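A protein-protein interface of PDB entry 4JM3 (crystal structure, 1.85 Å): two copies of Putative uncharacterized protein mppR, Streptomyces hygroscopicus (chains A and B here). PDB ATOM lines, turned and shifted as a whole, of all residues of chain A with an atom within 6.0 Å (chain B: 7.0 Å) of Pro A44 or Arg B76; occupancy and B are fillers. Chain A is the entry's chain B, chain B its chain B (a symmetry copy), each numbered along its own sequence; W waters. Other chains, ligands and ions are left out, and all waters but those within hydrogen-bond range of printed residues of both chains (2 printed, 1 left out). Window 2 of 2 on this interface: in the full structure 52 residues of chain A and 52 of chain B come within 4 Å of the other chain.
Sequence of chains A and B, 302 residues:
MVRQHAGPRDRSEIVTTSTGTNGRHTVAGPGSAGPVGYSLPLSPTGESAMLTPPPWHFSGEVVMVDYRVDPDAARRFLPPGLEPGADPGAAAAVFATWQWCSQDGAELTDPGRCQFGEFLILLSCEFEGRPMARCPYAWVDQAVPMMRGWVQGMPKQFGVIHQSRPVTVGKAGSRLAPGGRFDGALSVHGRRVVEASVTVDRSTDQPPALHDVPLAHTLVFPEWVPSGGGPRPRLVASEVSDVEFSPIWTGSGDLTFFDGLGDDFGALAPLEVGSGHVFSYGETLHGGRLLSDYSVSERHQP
OG1 of Thr A45 sits at hydrogen-bond distance from N of Glu A47, at 3.2 Å. The side-chain hydroxyl (OG) of Ser A43 lies within hydrogen-bond range of the backbone NH (N) of Gly A46 (3.1 Å). The side-chain hydroxyl of Ser A43 sits at hydrogen-bond distance from the backbone NH of Glu A47. N of Ser A43 lies within hydrogen-bond range of O of Val A36 (2.8 Å).
Water W2 bridges the side-chain carboxylate (OE2) of Glu A47 and the backbone NH (N) of Phe B265. Water W1 lies within hydrogen-bond range of O of Leu B78 (2.8 Å), N of Gly A34 (3.2 Å) and O of Ala A33 (3.5 Å).
Of the 13 printed residues of chain B, 5 touch a printed residue of chain A. Printed residues of chain B that touch a printed residue of chain A: Arg B76, Phe B77, Leu B78, Pro B79 and Asp B264. Hydrophobic or aromatic side chains of chain B that line the printed part of chain A: Phe B77. Along chain A the printed residues that touch a printed residue of chain B span positions 35 to 47. Among the printed residues, 12 pairs touch across the chains.
The side-chain hydroxyl of Ser A43 is in hydrogen-bond range of the side-chain carboxylate of Asp B264. The side-chain carboxylate of Glu A47 lies within hydrogen-bond range of the backbone NH of Asp B264. The side-chain hydroxyl (OG1) of Thr A45 lies within hydrogen-bond range of the side-chain carboxylate (OD1) of Asp B264, at 2.9 Å. N of Pro A44 lies close to OD2 of Asp B264, 3.4 Å away.
No position is printed for both chains.
Among the printed residues, pairs that only touch across the chains: Pro A35 with Arg B76, Pro A35 with Phe B77, Pro A35 with Leu B78, Pro A35 with Pro B79, Leu A42 with Phe B77, Pro A44 with Arg B76, Pro A44 with Phe B77 and Gly A46 with Asp B264.
Pro A44 touches just these residues of chain B: Arg B76, Phe B77 and Asp B264. Arg B76 touches just these residues of chain A: Pro A35 and Pro A44. Of the printed residues of chain B, Glu A47 touches Asp B264. Of the printed residues of chain B, Pro A35 touches Arg B76 (3.7 Å), Phe B77 (3.6 Å), Leu B78 (3.9 Å) and Pro B79 (3.8 Å). Printed residues of chain B within 4 Å of Gly A46: Asp B264 (3.9 Å). Printed residues of chain A within 4 Å of Leu B78: Pro A35 (3.9 Å). Of the printed residues of chain B, Leu A42 touches Phe B77 (3.9 Å). Tyr B137 touches none of the printed residues of chain A. The nearest residue of chain B that does not touch Pro A44 is Ala B73 (5.3 Å). The nearest printed residue of chain A that does not touch Pro B79 is Gly A34 (4.1 Å).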
ATOM      1  N   ALA A  33      32.089  22.494  15.079  1.00  0.00           N
ATOM      2  CA  ALA A  33      32.798  21.251  15.394  1.00  0.00           C
ATOM      3  C   ALA A  33      31.912  20.002  15.307  1.00  0.00           C
ATOM      4  O   ALA A  33      32.063  19.186  14.389  1.00  0.00           O
ATOM      5  CB  ALA A  33      33.428  21.340  16.783  1.00  0.00           C
ATOM      6  N   GLY A  34      31.017  19.840  16.279  1.00  0.00           N
ATOM      7  CA  GLY A  34      30.172  18.649  16.365  1.00  0.00           C
ATOM      8  C   GLY A  34      29.463  18.370  15.065  1.00  0.00           C
ATOM      9  O   GLY A  34      29.600  19.125  14.080  1.00  0.00           O
ATOM     10  N   PRO A  35      28.691  17.279  15.030  1.00  0.00           N
ATOM     11  CA  PRO A  35      27.869  17.103  13.836  1.00  0.00           C
ATOM     12  C   PRO A  35      26.783  18.179  13.785  1.00  0.00           C
ATOM     13  O   PRO A  35      26.426  18.756  14.826  1.00  0.00           O
ATOM     14  CB  PRO A  35      27.264  15.701  14.032  1.00  0.00           C
ATOM     15  CG  PRO A  35      27.260  15.516  15.518  1.00  0.00           C
ATOM     16  CD  PRO A  35      28.467  16.227  16.034  1.00  0.00           C
ATOM     17  N   VAL A  36      26.254  18.419  12.587  1.00  0.00           N
ATOM     18  CA  VAL A  36      25.323  19.511  12.340  1.00  0.00           C
ATOM     19  C   VAL A  36      24.035  19.038  11.676  1.00  0.00           C
ATOM     20  O   VAL A  36      23.917  17.887  11.250  1.00  0.00           O
ATOM     21  CB  VAL A  36      25.975  20.568  11.425  1.00  0.00           C
ATOM     22  CG1 VAL A  36      27.201  21.116  12.089  1.00  0.00           C
ATOM     23  CG2 VAL A  36      26.318  19.976  10.049  1.00  0.00           C
ATOM     24  N   LEU A  42      21.719  14.655  13.563  1.00  0.00           N
ATOM     25  CA  LEU A  42      22.893  15.448  13.208  1.00  0.00           C
ATOM     26  C   LEU A  42      23.879  14.560  12.461  1.00  0.00           C
ATOM     27  O   LEU A  42      23.933  13.342  12.683  1.00  0.00           O
ATOM     28  CB  LEU A  42      23.563  16.004  14.477  1.00  0.00           C
ATOM     29  CG  LEU A  42      22.675  16.797  15.437  1.00  0.00           C
ATOM     30  CD1 LEU A  42      23.436  17.194  16.698  1.00  0.00           C
ATOM     31  CD2 LEU A  42      22.098  18.020  14.781  1.00  0.00           C
ATOM     32  N   SER A  43      24.672  15.162  11.584  1.00  0.00           N
ATOM     33  CA  SER A  43      25.654  14.404  10.828  1.00  0.00           C
ATOM     34  C   SER A  43      26.778  15.320  10.428  1.00  0.00           C
ATOM     35  O   SER A  43      26.621  16.540  10.443  1.00  0.00           O
ATOM     36  CB  SER A  43      25.017  13.743   9.586  1.00  0.00           C
ATOM     37  OG  SER A  43      24.469  14.689   8.693  1.00  0.00           O
ATOM     38  N   PRO A  44      27.928  14.743  10.076  1.00  0.00           N
ATOM     39  CA  PRO A  44      29.070  15.592   9.699  1.00  0.00           C
ATOM     40  C   PRO A  44      28.783  16.637   8.598  1.00  0.00           C
ATOM     41  O   PRO A  44      29.269  17.758   8.735  1.00  0.00           O
ATOM     42  CB  PRO A  44      30.120  14.568   9.254  1.00  0.00           C
ATOM     43  CG  PRO A  44      29.820  13.375  10.129  1.00  0.00           C
ATOM     44  CD  PRO A  44      28.301  13.322  10.126  1.00  0.00           C
ATOM     45  N   THR A  45      28.019  16.312   7.552  1.00  0.00           N
ATOM     46  CA  THR A  45      27.705  17.297   6.509  1.00  0.00           C
ATOM     47  C   THR A  45      26.342  17.963   6.678  1.00  0.00           C
ATOM     48  O   THR A  45      26.036  18.937   5.992  1.00  0.00           O
ATOM     49  CB  THR A  45      27.700  16.662   5.101  1.00  0.00           C
ATOM     50  OG1 THR A  45      26.606  15.764   4.978  1.00  0.00           O
ATOM     51  CG2 THR A  45      28.992  15.909   4.850  1.00  0.00           C
ATOM     52  N   GLY A  46      25.513  17.442   7.576  1.00  0.00           N
ATOM     53  CA  GLY A  46      24.157  17.954   7.696  1.00  0.00           C
ATOM     54  C   GLY A  46      23.143  17.319   6.759  1.00  0.00           C
ATOM     55  O   GLY A  46      21.961  17.664   6.799  1.00  0.00           O
ATOM     56  N   GLU A  47      23.571  16.371   5.928  1.00  0.00           N
ATOM     57  CA  GLU A  47      22.660  15.786   4.932  1.00  0.00           C
ATOM     58  C   GLU A  47      21.626  14.836   5.541  1.00  0.00           C
ATOM     59  O   GLU A  47      20.551  14.661   4.971  1.00  0.00           O
ATOM     60  CB  GLU A  47      23.438  15.026   3.852  1.00  0.00           C
ATOM     61  CG  GLU A  47      24.057  13.755   4.373  1.00  0.00           C
ATOM     62  CD  GLU A  47      24.054  12.633   3.364  1.00  0.00           C
ATOM     63  OE1 GLU A  47      23.792  12.896   2.167  1.00  0.00           O
ATOM     64  OE2 GLU A  47      24.322  11.487   3.789  1.00  0.00           O
ATOM     65  N   PRO B  71      36.969   4.293  13.225  1.00  0.00           N
ATOM     66  CA  PRO B  71      36.950   5.172  14.412  1.00  0.00           C
ATOM     67  C   PRO B  71      36.980   6.656  14.066  1.00  0.00           C
ATOM     68  O   PRO B  71      36.444   7.482  14.796  1.00  0.00           O
ATOM     69  CB  PRO B  71      38.249   4.816  15.162  1.00  0.00           C
ATOM     70  CG  PRO B  71      38.814   3.603  14.480  1.00  0.00           C
ATOM     71  CD  PRO B  71      38.233   3.539  13.102  1.00  0.00           C
ATOM     72  N   ASP B  72      37.618   6.996  12.955  1.00  0.00           N
ATOM     73  CA  ASP B  72      37.693   8.390  12.551  1.00  0.00           C
ATOM     74  C   ASP B  72      36.330   8.872  12.062  1.00  0.00           C
ATOM     75  O   ASP B  72      35.947  10.018  12.292  1.00  0.00           O
ATOM     76  CB  ASP B  72      38.779   8.574  11.478  1.00  0.00           C
ATOM     77  CG  ASP B  72      40.167   8.276  12.010  1.00  0.00           C
ATOM     78  OD1 ASP B  72      40.431   8.600  13.184  1.00  0.00           O
ATOM     79  OD2 ASP B  72      41.002   7.715  11.270  1.00  0.00           O
ATOM     80  N   ALA B  73      35.588   7.977  11.429  1.00  0.00           N
ATOM     81  CA  ALA B  73      34.248   8.301  10.980  1.00  0.00           C
ATOM     82  C   ALA B  73      33.311   8.463  12.179  1.00  0.00           C
ATOM     83  O   ALA B  73      32.549   9.419  12.254  1.00  0.00           O
ATOM     84  CB  ALA B  73      33.734   7.231  10.063  1.00  0.00           C
ATOM     85  N   ALA B  74      33.363   7.514  13.100  1.00  0.00           N
ATOM     86  CA  ALA B  74      32.565   7.580  14.329  1.00  0.00           C
ATOM     87  C   ALA B  74      32.804   8.893  15.074  1.00  0.00           C
ATOM     88  O   ALA B  74      31.858   9.517  15.568  1.00  0.00           O
ATOM     89  CB  ALA B  74      32.874   6.400  15.231  1.00  0.00           C
ATOM     90  N   ARG B  75      34.060   9.321  15.145  1.00  0.00           N
ATOM     91  CA  ARG B  75      34.410  10.512  15.913  1.00  0.00           C
ATOM     92  C   ARG B  75      33.629  11.744  15.463  1.00  0.00           C
ATOM     93  O   ARG B  75      33.259  12.593  16.279  1.00  0.00           O
ATOM     94  CB  ARG B  75      35.912  10.796  15.827  1.00  0.00           C
ATOM     95  CG  ARG B  75      36.317  12.107  16.474  1.00  0.00           C
ATOM     96  CD  ARG B  75      37.845  12.219  16.593  1.00  0.00           C
ATOM     97  NE  ARG B  75      38.244  12.538  17.962  1.00  0.00           N
ATOM     98  CZ  ARG B  75      39.489  12.790  18.357  1.00  0.00           C
ATOM     99  NH1 ARG B  75      40.491  12.777  17.481  1.00  0.00           N
ATOM    100  NH2 ARG B  75      39.729  13.065  19.638  1.00  0.00           N
ATOM    101  N   ARG B  76      33.384  11.843  14.164  1.00  0.00           N
ATOM    102  CA  ARG B  76      32.711  13.003  13.622  1.00  0.00           C
ATOM    103  C   ARG B  76      31.218  13.079  14.001  1.00  0.00           C
ATOM    104  O   ARG B  76      30.585  14.121  13.811  1.00  0.00           O
ATOM    105  CB  ARG B  76      32.888  13.013  12.116  1.00  0.00           C
ATOM    106  CG  ARG B  76      34.368  13.049  11.737  1.00  0.00           C
ATOM    107  CD  ARG B  76      34.551  13.153  10.249  1.00  0.00           C
ATOM    108  NE  ARG B  76      34.003  14.405   9.729  1.00  0.00           N
ATOM    109  CZ  ARG B  76      33.738  14.625   8.446  1.00  0.00           C
ATOM    110  NH1 ARG B  76      33.968  13.677   7.542  1.00  0.00           N
ATOM    111  NH2 ARG B  76      33.232  15.791   8.069  1.00  0.00           N
ATOM    112  N   PHE B  77      30.670  11.989  14.538  1.00  0.00           N
ATOM    113  CA  PHE B  77      29.295  11.979  15.040  1.00  0.00           C
ATOM    114  C   PHE B  77      29.214  12.303  16.531  1.00  0.00           C
ATOM    115  O   PHE B  77      28.117  12.371  17.097  1.00  0.00           O
ATOM    116  CB  PHE B  77      28.617  10.620  14.786  1.00  0.00           C
ATOM    117  CG  PHE B  77      28.163  10.419  13.378  1.00  0.00           C
ATOM    118  CD1 PHE B  77      29.018   9.886  12.426  1.00  0.00           C
ATOM    119  CD2 PHE B  77      26.883  10.759  13.005  1.00  0.00           C
ATOM    120  CE1 PHE B  77      28.593   9.695  11.132  1.00  0.00           C
ATOM    121  CE2 PHE B  77      26.447  10.566  11.700  1.00  0.00           C
ATOM    122  CZ  PHE B  77      27.305  10.034  10.771  1.00  0.00           C
ATOM    123  N   LEU B  78      30.361  12.498  17.170  1.00  0.00           N
ATOM    124  CA  LEU B  78      30.384  12.798  18.598  1.00  0.00           C
ATOM    125  C   LEU B  78      30.488  14.293  18.799  1.00  0.00           C
ATOM    126  O   LEU B  78      31.483  14.905  18.392  1.00  0.00           O
ATOM    127  CB  LEU B  78      31.579  12.116  19.275  1.00  0.00           C
ATOM    128  CG  LEU B  78      31.694  10.588  19.123  1.00  0.00           C
ATOM    129  CD1 LEU B  78      32.936  10.070  19.849  1.00  0.00           C
ATOM    130  CD2 LEU B  78      30.433   9.857  19.617  1.00  0.00           C
ATOM    131  N   PRO B  79      29.476  14.901  19.439  1.00  0.00           N
ATOM    132  CA  PRO B  79      29.523  16.351  19.697  1.00  0.00           C
ATOM    133  C   PRO B  79      30.575  16.715  20.735  1.00  0.00           C
ATOM    134  O   PRO B  79      31.027  15.829  21.444  1.00  0.00           O
ATOM    135  CB  PRO B  79      28.130  16.656  20.247  1.00  0.00           C
ATOM    136  CG  PRO B  79      27.629  15.354  20.789  1.00  0.00           C
ATOM    137  CD  PRO B  79      28.252  14.274  19.972  1.00  0.00           C
ATOM    138  N   TYR B 137      21.877   7.306  14.803  1.00  0.00           N
ATOM    139  CA  TYR B 137      20.718   6.991  13.958  1.00  0.00           C
ATOM    140  C   TYR B 137      19.793   5.971  14.615  1.00  0.00           C
ATOM    141  O   TYR B 137      20.239   4.982  15.238  1.00  0.00           O
ATOM    142  CB  TYR B 137      21.153   6.388  12.621  1.00  0.00           C
ATOM    143  CG  TYR B 137      21.952   7.311  11.737  1.00  0.00           C
ATOM    144  CD1 TYR B 137      21.322   8.214  10.882  1.00  0.00           C
ATOM    145  CD2 TYR B 137      23.342   7.273  11.755  1.00  0.00           C
ATOM    146  CE1 TYR B 137      22.057   9.058  10.060  1.00  0.00           C
ATOM    147  CE2 TYR B 137      24.097   8.127  10.939  1.00  0.00           C
ATOM    148  CZ  TYR B 137      23.444   9.011  10.100  1.00  0.00           C
ATOM    149  OH  TYR B 137      24.197   9.828   9.285  1.00  0.00           O
ATOM    150  N   ASP B 264      26.684  10.062   4.570  1.00  0.00           N
ATOM    151  CA  ASP B 264      27.030  10.318   5.974  1.00  0.00           C
ATOM    152  C   ASP B 264      26.810   9.049   6.802  1.00  0.00           C
ATOM    153  O   ASP B 264      27.650   8.689   7.640  1.00  0.00           O
ATOM    154  CB  ASP B 264      26.234  11.494   6.550  1.00  0.00           C
ATOM    155  CG  ASP B 264      26.850  12.851   6.226  1.00  0.00           C
ATOM    156  OD1 ASP B 264      27.425  13.028   5.132  1.00  0.00           O
ATOM    157  OD2 ASP B 264      26.763  13.756   7.075  1.00  0.00           O
ATOM    158  N   PHE B 265      25.669   8.398   6.579  1.00  0.00           N
ATOM    159  CA  PHE B 265      25.331   7.146   7.246  1.00  0.00           C
ATOM    160  C   PHE B 265      26.280   6.038   6.794  1.00  0.00           C
ATOM    161  O   PHE B 265      26.748   5.244   7.608  1.00  0.00           O
ATOM    162  CB  PHE B 265      23.880   6.734   6.937  1.00  0.00           C
ATOM    163  CG  PHE B 265      23.497   5.391   7.512  1.00  0.00           C
ATOM    164  CD1 PHE B 265      23.043   5.287   8.823  1.00  0.00           C
ATOM    165  CD2 PHE B 265      23.609   4.237   6.757  1.00  0.00           C
ATOM    166  CE1 PHE B 265      22.707   4.057   9.363  1.00  0.00           C
ATOM    167  CE2 PHE B 265      23.271   3.005   7.288  1.00  0.00           C
ATOM    168  CZ  PHE B 265      22.821   2.912   8.595  1.00  0.00           C
ATOM    169  N   ALA B 267      29.323   6.039   6.030  1.00  0.00           N
ATOM    170  CA  ALA B 267      30.631   6.109   6.664  1.00  0.00           C
ATOM    171  C   ALA B 267      30.706   5.206   7.895  1.00  0.00           C
ATOM    172  O   ALA B 267      31.803   4.850   8.343  1.00  0.00           O
ATOM    173  CB  ALA B 267      30.940   7.541   7.054  1.00  0.00           C
HETATM  174  O   HOH W   1      32.578  17.156  17.173  1.00  0.00           O
HETATM  175  O   HOH W   2      23.219  10.114   5.617  1.00  0.00           O
